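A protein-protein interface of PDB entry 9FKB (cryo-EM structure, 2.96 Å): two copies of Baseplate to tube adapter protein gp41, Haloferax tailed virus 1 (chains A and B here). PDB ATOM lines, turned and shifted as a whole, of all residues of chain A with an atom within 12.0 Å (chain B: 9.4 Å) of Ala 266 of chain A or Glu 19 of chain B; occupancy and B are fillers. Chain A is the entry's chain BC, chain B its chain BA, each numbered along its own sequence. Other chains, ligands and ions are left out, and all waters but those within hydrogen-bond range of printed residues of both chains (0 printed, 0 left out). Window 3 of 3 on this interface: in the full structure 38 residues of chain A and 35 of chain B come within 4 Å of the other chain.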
ATOM      1  N   GLU A 211     -27.373  13.380  -2.629  1.00  0.00           N
ATOM      2  CA  GLU A 211     -27.445  14.818  -2.378  1.00  0.00           C
ATOM      3  C   GLU A 211     -28.391  15.484  -3.383  1.00  0.00           C
ATOM      4  O   GLU A 211     -28.272  15.268  -4.586  1.00  0.00           O
ATOM      5  CB  GLU A 211     -26.048  15.446  -2.372  1.00  0.00           C
ATOM      6  CG  GLU A 211     -25.111  14.794  -1.363  1.00  0.00           C
ATOM      7  CD  GLU A 211     -23.810  15.526  -1.050  1.00  0.00           C
ATOM      8  OE1 GLU A 211     -23.575  16.601  -1.640  1.00  0.00           O
ATOM      9  OE2 GLU A 211     -23.017  15.038  -0.213  1.00  0.00           O
ATOM     10  N   GLN A 262     -32.360  14.686   6.608  1.00  0.00           N
ATOM     11  CA  GLN A 262     -31.848  15.803   5.833  1.00  0.00           C
ATOM     12  C   GLN A 262     -30.705  16.436   6.609  1.00  0.00           C
ATOM     13  O   GLN A 262     -30.791  16.576   7.828  1.00  0.00           O
ATOM     14  CB  GLN A 262     -32.913  16.865   5.587  1.00  0.00           C
ATOM     15  CG  GLN A 262     -33.854  16.455   4.471  1.00  0.00           C
ATOM     16  CD  GLN A 262     -35.178  17.180   4.447  1.00  0.00           C
ATOM     17  OE1 GLN A 262     -36.149  16.693   3.869  1.00  0.00           O
ATOM     18  NE2 GLN A 262     -35.232  18.339   5.090  1.00  0.00           N
ATOM     19  N   VAL A 263     -29.656  16.831   5.882  1.00  0.00           N
ATOM     20  CA  VAL A 263     -28.496  17.476   6.474  1.00  0.00           C
ATOM     21  C   VAL A 263     -28.124  18.724   5.678  1.00  0.00           C
ATOM     22  O   VAL A 263     -27.832  18.663   4.483  1.00  0.00           O
ATOM     23  CB  VAL A 263     -27.329  16.479   6.618  1.00  0.00           C
ATOM     24  CG1 VAL A 263     -25.980  17.177   6.747  1.00  0.00           C
ATOM     25  CG2 VAL A 263     -27.550  15.583   7.827  1.00  0.00           C
ATOM     26  N   HIS A 264     -28.111  19.844   6.406  1.00  0.00           N
ATOM     27  CA  HIS A 264     -27.717  21.152   5.926  1.00  0.00           C
ATOM     28  C   HIS A 264     -26.361  21.507   6.546  1.00  0.00           C
ATOM     29  O   HIS A 264     -26.217  21.428   7.768  1.00  0.00           O
ATOM     30  CB  HIS A 264     -28.776  22.140   6.400  1.00  0.00           C
ATOM     31  CG  HIS A 264     -30.101  22.085   5.703  1.00  0.00           C
ATOM     32  ND1 HIS A 264     -30.938  20.977   5.678  1.00  0.00           N
ATOM     33  CD2 HIS A 264     -30.768  23.065   5.057  1.00  0.00           C
ATOM     34  CE1 HIS A 264     -32.037  21.274   5.022  1.00  0.00           C
ATOM     35  NE2 HIS A 264     -31.947  22.542   4.619  1.00  0.00           N
ATOM     36  N   GLN A 265     -25.389  21.905   5.708  1.00  0.00           N
ATOM     37  CA  GLN A 265     -24.009  22.046   6.167  1.00  0.00           C
ATOM     38  C   GLN A 265     -23.482  23.459   5.954  1.00  0.00           C
ATOM     39  O   GLN A 265     -23.875  24.136   5.019  1.00  0.00           O
ATOM     40  CB  GLN A 265     -23.090  21.040   5.479  1.00  0.00           C
ATOM     41  CG  GLN A 265     -23.315  19.615   5.954  1.00  0.00           C
ATOM     42  CD  GLN A 265     -22.598  18.585   5.112  1.00  0.00           C
ATOM     43  OE1 GLN A 265     -23.203  17.905   4.289  1.00  0.00           O
ATOM     44  NE2 GLN A 265     -21.291  18.464   5.289  1.00  0.00           N
ATOM     45  N   ALA A 266     -22.559  23.881   6.822  1.00  0.00           N
ATOM     46  CA  ALA A 266     -21.884  25.167   6.704  1.00  0.00           C
ATOM     47  C   ALA A 266     -21.278  25.356   5.307  1.00  0.00           C
ATOM     48  O   ALA A 266     -20.584  24.474   4.802  1.00  0.00           O
ATOM     49  CB  ALA A 266     -20.844  25.269   7.798  1.00  0.00           C
ATOM     50  N   GLY A 267     -21.606  26.484   4.648  1.00  0.00           N
ATOM     51  CA  GLY A 267     -21.002  26.851   3.378  1.00  0.00           C
ATOM     52  C   GLY A 267     -21.528  26.077   2.162  1.00  0.00           C
ATOM     53  O   GLY A 267     -21.031  26.286   1.054  1.00  0.00           O
ATOM     54  N   ARG A 268     -22.544  25.214   2.333  1.00  0.00           N
ATOM     55  CA  ARG A 268     -23.121  24.448   1.234  1.00  0.00           C
ATOM     56  C   ARG A 268     -24.463  25.057   0.813  1.00  0.00           C
ATOM     57  O   ARG A 268     -25.358  25.270   1.627  1.00  0.00           O
ATOM     58  CB  ARG A 268     -23.267  22.964   1.603  1.00  0.00           C
ATOM     59  CG  ARG A 268     -21.951  22.263   1.914  1.00  0.00           C
ATOM     60  CD  ARG A 268     -22.027  20.762   1.715  1.00  0.00           C
ATOM     61  NE  ARG A 268     -20.752  20.089   1.919  1.00  0.00           N
ATOM     62  CZ  ARG A 268     -20.515  18.789   1.737  1.00  0.00           C
ATOM     63  NH1 ARG A 268     -19.304  18.304   1.953  1.00  0.00           N
ATOM     64  NH2 ARG A 268     -21.479  17.968   1.352  1.00  0.00           N
ATOM     65  N   GLY A 269     -24.636  25.277  -0.498  1.00  0.00           N
ATOM     66  CA  GLY A 269     -25.891  25.780  -1.054  1.00  0.00           C
ATOM     67  C   GLY A 269     -26.956  24.719  -1.375  1.00  0.00           C
ATOM     68  O   GLY A 269     -27.902  25.049  -2.097  1.00  0.00           O
ATOM     69  N   TRP A 270     -26.799  23.484  -0.847  1.00  0.00           N
ATOM     70  CA  TRP A 270     -27.672  22.347  -1.130  1.00  0.00           C
ATOM     71  C   TRP A 270     -27.670  21.317   0.009  1.00  0.00           C
ATOM     72  O   TRP A 270     -26.846  21.381   0.915  1.00  0.00           O
ATOM     73  CB  TRP A 270     -27.270  21.703  -2.461  1.00  0.00           C
ATOM     74  CG  TRP A 270     -26.055  20.832  -2.352  1.00  0.00           C
ATOM     75  CD1 TRP A 270     -26.054  19.490  -2.127  1.00  0.00           C
ATOM     76  CD2 TRP A 270     -24.660  21.236  -2.392  1.00  0.00           C
ATOM     77  NE1 TRP A 270     -24.767  19.034  -2.055  1.00  0.00           N
ATOM     78  CE2 TRP A 270     -23.878  20.073  -2.196  1.00  0.00           C
ATOM     79  CE3 TRP A 270     -23.983  22.453  -2.589  1.00  0.00           C
ATOM     80  CZ2 TRP A 270     -22.470  20.096  -2.224  1.00  0.00           C
ATOM     81  CZ3 TRP A 270     -22.599  22.488  -2.595  1.00  0.00           C
ATOM     82  CH2 TRP A 270     -21.851  21.317  -2.425  1.00  0.00           C
ATOM     83  N   VAL A 271     -28.593  20.340  -0.068  1.00  0.00           N
ATOM     84  CA  VAL A 271     -28.927  19.454   1.046  1.00  0.00           C
ATOM     85  C   VAL A 271     -28.448  18.024   0.807  1.00  0.00           C
ATOM     86  O   VAL A 271     -28.713  17.399  -0.217  1.00  0.00           O
ATOM     87  CB  VAL A 271     -30.429  19.507   1.391  1.00  0.00           C
ATOM     88  CG1 VAL A 271     -30.818  18.503   2.465  1.00  0.00           C
ATOM     89  CG2 VAL A 271     -30.798  20.900   1.868  1.00  0.00           C
ATOM     90  N   THR A 272     -27.746  17.497   1.809  1.00  0.00           N
ATOM     91  CA  THR A 272     -27.316  16.107   1.862  1.00  0.00           C
ATOM     92  C   THR A 272     -28.460  15.253   2.409  1.00  0.00           C
ATOM     93  O   THR A 272     -29.138  15.669   3.347  1.00  0.00           O
ATOM     94  CB  THR A 272     -26.088  15.962   2.778  1.00  0.00           C
ATOM     95  OG1 THR A 272     -25.059  16.837   2.315  1.00  0.00           O
ATOM     96  CG2 THR A 272     -25.507  14.564   2.809  1.00  0.00           C
ATOM     97  N   VAL B   2     -28.638  34.835   8.953  1.00  0.00           N
ATOM     98  CA  VAL B   2     -27.606  34.164   9.816  1.00  0.00           C
ATOM     99  C   VAL B   2     -28.307  33.245  10.825  1.00  0.00           C
ATOM    100  O   VAL B   2     -27.910  32.096  10.981  1.00  0.00           O
ATOM    101  CB  VAL B   2     -26.683  35.173  10.541  1.00  0.00           C
ATOM    102  CG1 VAL B   2     -25.525  34.483  11.244  1.00  0.00           C
ATOM    103  CG2 VAL B   2     -26.156  36.280   9.629  1.00  0.00           C
ATOM    104  N   PRO B  16     -27.203  31.905  15.734  1.00  0.00           N
ATOM    105  CA  PRO B  16     -26.415  31.782  14.506  1.00  0.00           C
ATOM    106  C   PRO B  16     -26.143  30.333  14.089  1.00  0.00           C
ATOM    107  O   PRO B  16     -25.469  29.589  14.782  1.00  0.00           O
ATOM    108  CB  PRO B  16     -25.093  32.511  14.829  1.00  0.00           C
ATOM    109  CG  PRO B  16     -25.413  33.429  15.993  1.00  0.00           C
ATOM    110  CD  PRO B  16     -26.467  32.657  16.756  1.00  0.00           C
ATOM    111  N   LEU B  17     -26.692  29.930  12.938  1.00  0.00           N
ATOM    112  CA  LEU B  17     -26.358  28.653  12.309  1.00  0.00           C
ATOM    113  C   LEU B  17     -25.059  28.833  11.525  1.00  0.00           C
ATOM    114  O   LEU B  17     -25.065  28.899  10.293  1.00  0.00           O
ATOM    115  CB  LEU B  17     -27.500  28.151  11.415  1.00  0.00           C
ATOM    116  CG  LEU B  17     -28.825  27.853  12.115  1.00  0.00           C
ATOM    117  CD1 LEU B  17     -29.894  27.499  11.097  1.00  0.00           C
ATOM    118  CD2 LEU B  17     -28.704  26.726  13.124  1.00  0.00           C
ATOM    119  N   VAL B  18     -23.945  28.936  12.268  1.00  0.00           N
ATOM    120  CA  VAL B  18     -22.629  29.209  11.695  1.00  0.00           C
ATOM    121  C   VAL B  18     -21.564  28.299  12.315  1.00  0.00           C
ATOM    122  O   VAL B  18     -21.554  28.105  13.535  1.00  0.00           O
ATOM    123  CB  VAL B  18     -22.247  30.698  11.809  1.00  0.00           C
ATOM    124  CG1 VAL B  18     -23.324  31.608  11.253  1.00  0.00           C
ATOM    125  CG2 VAL B  18     -21.923  31.105  13.232  1.00  0.00           C
ATOM    126  N   GLU B  19     -20.672  27.754  11.456  1.00  0.00           N
ATOM    127  CA  GLU B  19     -19.662  26.769  11.853  1.00  0.00           C
ATOM    128  C   GLU B  19     -18.388  26.814  10.995  1.00  0.00           C
ATOM    129  O   GLU B  19     -18.415  27.223   9.835  1.00  0.00           O
ATOM    130  CB  GLU B  19     -20.249  25.350  11.881  1.00  0.00           C
ATOM    131  CG  GLU B  19     -20.673  24.860  13.266  1.00  0.00           C
ATOM    132  CD  GLU B  19     -19.550  24.661  14.279  1.00  0.00           C
ATOM    133  OE1 GLU B  19     -18.492  25.353  14.190  1.00  0.00           O
ATOM    134  OE2 GLU B  19     -19.741  23.825  15.191  1.00  0.00           O
ATOM    135  N   GLU B  20     -17.269  26.345  11.583  1.00  0.00           N
ATOM    136  CA  GLU B  20     -15.968  26.187  10.927  1.00  0.00           C
ATOM    137  C   GLU B  20     -16.012  25.066   9.876  1.00  0.00           C
ATOM    138  O   GLU B  20     -16.518  23.975  10.146  1.00  0.00           O
ATOM    139  CB  GLU B  20     -14.899  25.929  12.004  1.00  0.00           C
ATOM    140  CG  GLU B  20     -13.509  25.474  11.533  1.00  0.00           C
ATOM    141  CD  GLU B  20     -12.554  26.524  10.980  1.00  0.00           C
ATOM    142  OE1 GLU B  20     -13.009  27.647  10.673  1.00  0.00           O
ATOM    143  OE2 GLU B  20     -11.343  26.218  10.862  1.00  0.00           O
ATOM    144  N   GLY B  21     -15.433  25.308   8.685  1.00  0.00           N
ATOM    145  CA  GLY B  21     -15.310  24.291   7.640  1.00  0.00           C
ATOM    146  C   GLY B  21     -16.655  23.813   7.077  1.00  0.00           C
ATOM    147  O   GLY B  21     -17.553  24.623   6.856  1.00  0.00           O
ATOM    148  N   GLY B  22     -16.801  22.488   6.871  1.00  0.00           N
ATOM    149  CA  GLY B  22     -17.982  21.895   6.242  1.00  0.00           C
ATOM    150  C   GLY B  22     -18.895  21.118   7.201  1.00  0.00           C
ATOM    151  O   GLY B  22     -19.618  20.210   6.776  1.00  0.00           O
ATOM    152  N   GLU B  23     -18.897  21.500   8.486  1.00  0.00           N
ATOM    153  CA  GLU B  23     -19.644  20.818   9.546  1.00  0.00           C
ATOM    154  C   GLU B  23     -21.170  20.913   9.369  1.00  0.00           C
ATOM    155  O   GLU B  23     -21.695  21.845   8.751  1.00  0.00           O
ATOM    156  CB  GLU B  23     -19.223  21.351  10.920  1.00  0.00           C
ATOM    157  CG  GLU B  23     -17.782  21.009  11.307  1.00  0.00           C
ATOM    158  CD  GLU B  23     -17.458  19.527  11.466  1.00  0.00           C
ATOM    159  OE1 GLU B  23     -18.400  18.736  11.717  1.00  0.00           O
ATOM    160  OE2 GLU B  23     -16.272  19.163  11.303  1.00  0.00           O
ATOM    161  N   ILE B  24     -21.887  19.943   9.958  1.00  0.00           N
ATOM    162  CA  ILE B  24     -23.349  19.939   9.986  1.00  0.00           C
ATOM    163  C   ILE B  24     -23.857  21.101  10.842  1.00  0.00           C
ATOM    164  O   ILE B  24     -23.409  21.276  11.975  1.00  0.00           O
ATOM    165  CB  ILE B  24     -23.891  18.577  10.486  1.00  0.00           C
ATOM    166  CG1 ILE B  24     -23.405  17.425   9.595  1.00  0.00           C
ATOM    167  CG2 ILE B  24     -25.414  18.611  10.637  1.00  0.00           C
ATOM    168  CD1 ILE B  24     -23.444  16.025  10.227  1.00  0.00           C
ATOM    169  N   LEU B  25     -24.831  21.857  10.301  1.00  0.00           N
ATOM    170  CA  LEU B  25     -25.452  22.983  10.994  1.00  0.00           C
ATOM    171  C   LEU B  25     -26.898  22.701  11.390  1.00  0.00           C
ATOM    172  O   LEU B  25     -27.315  23.068  12.490  1.00  0.00           O
ATOM    173  CB  LEU B  25     -25.402  24.214  10.098  1.00  0.00           C
ATOM    174  CG  LEU B  25     -24.063  24.928  10.091  1.00  0.00           C
ATOM    175  CD1 LEU B  25     -24.095  25.996   9.021  1.00  0.00           C
ATOM    176  CD2 LEU B  25     -23.791  25.568  11.445  1.00  0.00           C
ATOM    177  N   LEU B  26     -27.657  22.091  10.473  1.00  0.00           N
ATOM    178  CA  LEU B  26     -29.043  21.748  10.730  1.00  0.00           C
ATOM    179  C   LEU B  26     -29.314  20.375  10.130  1.00  0.00           C
ATOM    180  O   LEU B  26     -28.990  20.119   8.971  1.00  0.00           O
ATOM    181  CB  LEU B  26     -29.941  22.813  10.105  1.00  0.00           C
ATOM    182  CG  LEU B  26     -31.337  22.964  10.707  1.00  0.00           C
ATOM    183  CD1 LEU B  26     -32.070  24.116  10.024  1.00  0.00           C
ATOM    184  CD2 LEU B  26     -32.168  21.699  10.571  1.00  0.00           C
ATOM    185  N   LEU B  60     -29.872  21.326  15.719  1.00  0.00           N
ATOM    186  CA  LEU B  60     -29.295  22.620  15.370  1.00  0.00           C
ATOM    187  C   LEU B  60     -27.922  22.756  16.032  1.00  0.00           C
ATOM    188  O   LEU B  60     -27.733  22.374  17.191  1.00  0.00           O
ATOM    189  CB  LEU B  60     -30.236  23.741  15.829  1.00  0.00           C
ATOM    190  CG  LEU B  60     -31.305  24.197  14.835  1.00  0.00           C
ATOM    191  CD1 LEU B  60     -32.372  23.153  14.582  1.00  0.00           C
ATOM    192  CD2 LEU B  60     -31.987  25.460  15.336  1.00  0.00           C
ATOM    193  N   VAL B  61     -26.959  23.318  15.287  1.00  0.00           N
ATOM    194  CA  VAL B  61     -25.611  23.608  15.777  1.00  0.00           C
ATOM    195  C   VAL B  61     -25.290  25.068  15.474  1.00  0.00           C
ATOM    196  O   VAL B  61     -25.640  25.557  14.410  1.00  0.00           O
ATOM    197  CB  VAL B  61     -24.554  22.669  15.149  1.00  0.00           C
ATOM    198  CG1 VAL B  61     -23.164  22.901  15.732  1.00  0.00           C
ATOM    199  CG2 VAL B  61     -24.919  21.202  15.317  1.00  0.00           C
ATOM    200  N   GLY B  62     -24.621  25.752  16.410  1.00  0.00           N
ATOM    201  CA  GLY B  62     -24.196  27.123  16.210  1.00  0.00           C
ATOM    202  C   GLY B  62     -23.119  27.553  17.206  1.00  0.00           C
ATOM    203  O   GLY B  62     -22.687  26.789  18.068  1.00  0.00           O
ATOM    204  N   LYS B  63     -22.696  28.806  17.062  1.00  0.00           N
ATOM    205  CA  LYS B  63     -21.779  29.455  17.981  1.00  0.00           C
ATOM    206  C   LYS B  63     -22.434  30.738  18.475  1.00  0.00           C
ATOM    207  O   LYS B  63     -22.924  31.525  17.666  1.00  0.00           O
ATOM    208  CB  LYS B  63     -20.452  29.740  17.272  1.00  0.00           C
ATOM    209  CG  LYS B  63     -19.518  28.542  17.253  1.00  0.00           C
ATOM    210  CD  LYS B  63     -18.455  28.629  16.175  1.00  0.00           C
ATOM    211  CE  LYS B  63     -17.207  27.804  16.442  1.00  0.00           C
ATOM    212  NZ  LYS B  63     -17.490  26.354  16.567  1.00  0.00           N
ATOM    213  N   LEU B  64     -22.444  30.948  19.799  1.00  0.00           N
ATOM    214  CA  LEU B  64     -22.949  32.187  20.369  1.00  0.00           C
ATOM    215  C   LEU B  64     -21.784  33.077  20.786  1.00  0.00           C
ATOM    216  O   LEU B  64     -20.782  32.610  21.330  1.00  0.00           O
ATOM    217  CB  LEU B  64     -23.919  31.899  21.522  1.00  0.00           C
ATOM    218  CG  LEU B  64     -25.316  31.437  21.092  1.00  0.00           C
ATOM    219  CD1 LEU B  64     -26.138  31.038  22.309  1.00  0.00           C
ATOM    220  CD2 LEU B  64     -26.068  32.526  20.329  1.00  0.00           C
ATOM    221  N   TYR B  65     -21.940  34.379  20.514  1.00  0.00           N
ATOM    222  CA  TYR B  65     -20.886  35.369  20.694  1.00  0.00           C
ATOM    223  C   TYR B  65     -20.926  36.102  22.045  1.00  0.00           C
ATOM    224  O   TYR B  65     -20.045  36.924  22.316  1.00  0.00           O
ATOM    225  CB  TYR B  65     -20.952  36.364  19.540  1.00  0.00           C
ATOM    226  CG  TYR B  65     -20.827  35.737  18.174  1.00  0.00           C
ATOM    227  CD1 TYR B  65     -19.725  34.946  17.862  1.00  0.00           C
ATOM    228  CD2 TYR B  65     -21.791  35.942  17.196  1.00  0.00           C
ATOM    229  CE1 TYR B  65     -19.576  34.365  16.609  1.00  0.00           C
ATOM    230  CE2 TYR B  65     -21.650  35.387  15.929  1.00  0.00           C
ATOM    231  CZ  TYR B  65     -20.542  34.601  15.637  1.00  0.00           C
ATOM    232  OH  TYR B  65     -20.396  34.057  14.389  1.00  0.00           O
ATOM    233  N   GLU B 113     -20.883  24.888  25.491  1.00  0.00           N
ATOM    234  CA  GLU B 113     -19.484  24.587  25.779  1.00  0.00           C
ATOM    235  C   GLU B 113     -18.606  25.835  25.767  1.00  0.00           C
ATOM    236  O   GLU B 113     -18.693  26.677  24.887  1.00  0.00           O
ATOM    237  CB  GLU B 113     -18.877  23.564  24.821  1.00  0.00           C
ATOM    238  CG  GLU B 113     -19.767  22.372  24.500  1.00  0.00           C
ATOM    239  CD  GLU B 113     -19.151  21.361  23.542  1.00  0.00           C
ATOM    240  OE1 GLU B 113     -17.972  20.986  23.757  1.00  0.00           O
ATOM    241  OE2 GLU B 113     -19.846  20.944  22.576  1.00  0.00           O
ATOM    242  N   ARG B 118     -11.058  30.085  23.677  1.00  0.00           N
ATOM    243  CA  ARG B 118     -12.046  30.655  22.762  1.00  0.00           C
ATOM    244  C   ARG B 118     -12.978  31.666  23.452  1.00  0.00           C
ATOM    245  O   ARG B 118     -14.196  31.528  23.396  1.00  0.00           O
ATOM    246  CB  ARG B 118     -12.794  29.528  22.042  1.00  0.00           C
ATOM    247  CG  ARG B 118     -11.925  28.345  21.620  1.00  0.00           C
ATOM    248  CD  ARG B 118     -12.609  27.335  20.730  1.00  0.00           C
ATOM    249  NE  ARG B 118     -12.533  27.536  19.285  1.00  0.00           N
ATOM    250  CZ  ARG B 118     -12.941  26.657  18.389  1.00  0.00           C
ATOM    251  NH1 ARG B 118     -12.839  26.934  17.097  1.00  0.00           N
ATOM    252  NH2 ARG B 118     -13.438  25.491  18.770  1.00  0.00           N
ATOM    253  N   LEU B 121     -16.526  32.794  22.203  1.00  0.00           N
ATOM    254  CA  LEU B 121     -17.145  31.698  21.462  1.00  0.00           C
ATOM    255  C   LEU B 121     -17.712  30.688  22.452  1.00  0.00           C
ATOM    256  O   LEU B 121     -16.966  30.059  23.195  1.00  0.00           O
ATOM    257  CB  LEU B 121     -16.130  31.014  20.539  1.00  0.00           C
ATOM    258  CG  LEU B 121     -15.825  31.723  19.222  1.00  0.00           C
ATOM    259  CD1 LEU B 121     -14.588  31.095  18.590  1.00  0.00           C
ATOM    260  CD2 LEU B 121     -17.020  31.636  18.267  1.00  0.00           C
ATOM    261  N   VAL B 122     -19.035  30.498  22.417  1.00  0.00           N
ATOM    262  CA  VAL B 122     -19.684  29.383  23.085  1.00  0.00           C
ATOM    263  C   VAL B 122     -20.175  28.442  21.988  1.00  0.00           C
ATOM    264  O   VAL B 122     -20.936  28.861  21.123  1.00  0.00           O
ATOM    265  CB  VAL B 122     -20.846  29.869  23.980  1.00  0.00           C
ATOM    266  CG1 VAL B 122     -21.531  28.719  24.696  1.00  0.00           C
ATOM    267  CG2 VAL B 122     -20.381  30.881  25.008  1.00  0.00           C
ATOM    268  N   ASP B 123     -19.733  27.180  21.999  1.00  0.00           N
ATOM    269  CA  ASP B 123     -20.288  26.184  21.091  1.00  0.00           C
ATOM    270  C   ASP B 123     -21.643  25.724  21.611  1.00  0.00           C
ATOM    271  O   ASP B 123     -21.797  25.451  22.802  1.00  0.00           O
ATOM    272  CB  ASP B 123     -19.401  24.945  20.947  1.00  0.00           C
ATOM    273  CG  ASP B 123     -18.155  25.129  20.094  1.00  0.00           C
ATOM    274  OD1 ASP B 123     -18.189  25.958  19.165  1.00  0.00           O
ATOM    275  OD2 ASP B 123     -17.160  24.413  20.347  1.00  0.00           O
ATOM    276  N   VAL B 124     -22.602  25.595  20.693  1.00  0.00           N
ATOM    277  CA  VAL B 124     -23.976  25.256  21.041  1.00  0.00           C
ATOM    278  C   VAL B 124     -24.444  24.076  20.195  1.00  0.00           C
ATOM    279  O   VAL B 124     -24.318  24.113  18.970  1.00  0.00           O
ATOM    280  CB  VAL B 124     -24.925  26.465  20.864  1.00  0.00           C
ATOM    281  CG1 VAL B 124     -26.327  26.146  21.339  1.00  0.00           C
ATOM    282  CG2 VAL B 124     -24.438  27.703  21.596  1.00  0.00           C
ATOM    283  N   SER B 125     -25.074  23.087  20.850  1.00  0.00           N
ATOM    284  CA  SER B 125     -25.808  22.025  20.168  1.00  0.00           C
ATOM    285  C   SER B 125     -27.213  21.870  20.769  1.00  0.00           C
ATOM    286  O   SER B 125     -27.362  21.841  21.990  1.00  0.00           O
ATOM    287  CB  SER B 125     -25.031  20.722  20.185  1.00  0.00           C
ATOM    288  OG  SER B 125     -23.738  20.889  19.618  1.00  0.00           O
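The backbone carbonyl oxygen of Gly 22 of chain B is in hydrogen-bond range of the side-chain amide nitrogen of Gln 265 of chain A, at 2.8 Å. The backbone carbonyl oxygen of Glu 23 of chain B lies within hydrogen-bond range of the backbone NH of Ala 266 of chain A (2.9 Å). O of His 264 of chain A lies within hydrogen-bond range of N of Leu 25 of chain B (2.9 Å). The backbone NH (N) of His 264 of chain A is in hydrogen-bond range of the backbone carbonyl oxygen (O) of Leu 26 of chain B, at 2.7 Å.
Of the 25 printed residues of chain B, 7 touch a printed residue of chain A. Hydrophobic or aromatic side chains of chain A that line the printed part of chain B: Val 263, His 264 and Ala 266. Among the printed residues, 12 pairs touch across the chains. Among the printed residues, no Asp or Glu carboxylate lies within 4 Å of a Lys or Arg side-chain nitrogen of the other chain.
Among the printed residues, merely in contact across the chains: Val 263 of chain A with Ile 24 of chain B, Val 263 of chain A with Leu 26 of chain B, His 264 of chain A with Ile 24 of chain B, Gln 265 of chain A with Glu 23 of chain B, Ala 266 of chain A with Glu 19 of chain B, Ala 266 of chain A with Gly 21 of chain B, Ala 266 of chain A with Gly 22 of chain B and Ala 266 of chain A with Leu 25 of chain B.
The side-chain carboxylate (OE1) of Glu 19 of chain B is in salt-bridge range of the side-chain amino group (NZ) of Lys 63 of chain B (2.8 Å). N of Val 61 of chain B is in hydrogen-bond range of O of Leu 25 of chain B (2.8 Å). N of Val 263 of chain A is in hydrogen-bond range of O of Thr 272 of chain A, 2.8 Å away. NH2 of Arg 268 of chain A lies within hydrogen-bond range of OE1 of Gln 265 of chain A, at 3.4 Å. OG1 of Thr 272 of chain A is in hydrogen-bond range of OE1 of Gln 265 of chain A (2.9 Å).
No position is printed for both chains. Of the 12 pairs that touch across the chains among the printed residues, none has its exchanged pair printed and touching as well.
Of chain A, only Ala 266 (3.7 Å) comes within 4 Å of Glu 19 of chain B. No residue of chain A comes within 4 Å of Val 18 of chain B. No residue of chain A comes within 4 Å of Glu 20 of chain B. Of chain A, only Gln 265 (2.8 Å) and Ala 266 (3.9 Å) come within 4 Å of Gly 22 of chain B. Of chain A, only Gln 265 and Ala 266 come within 4 Å of Glu 23 of chain B. Printed residues of chain A within 4 Å of Leu 25 of chain B: His 264 and Ala 266. No residue of chain A comes within 4 Å of Gly 62 of chain B. No residue of chain A comes within 4 Å of Lys 63 of chain B. Of the printed residues of chain B, Val 263 of chain A touches Ile 24 (3.8 Å) and Leu 26 (3.7 Å). Of the printed residues of chain A, Ile 24 of chain B touches Val 263 (3.8 Å) and His 264 (3.9 Å). Of the printed residues of chain B, Gln 265 of chain A touches Gly 22 (2.8 Å) and Glu 23 (3.5 Å). Printed residues of chain B within 4 Å of His 264 of chain A: Ile 24 (3.9 Å), Leu 25 (2.9 Å) and Leu 26 (2.7 Å). Of the printed residues of chain A, Leu 26 of chain B touches Val 263 and His 264. Val 271 of chain A touches none of the printed residues of chain B.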
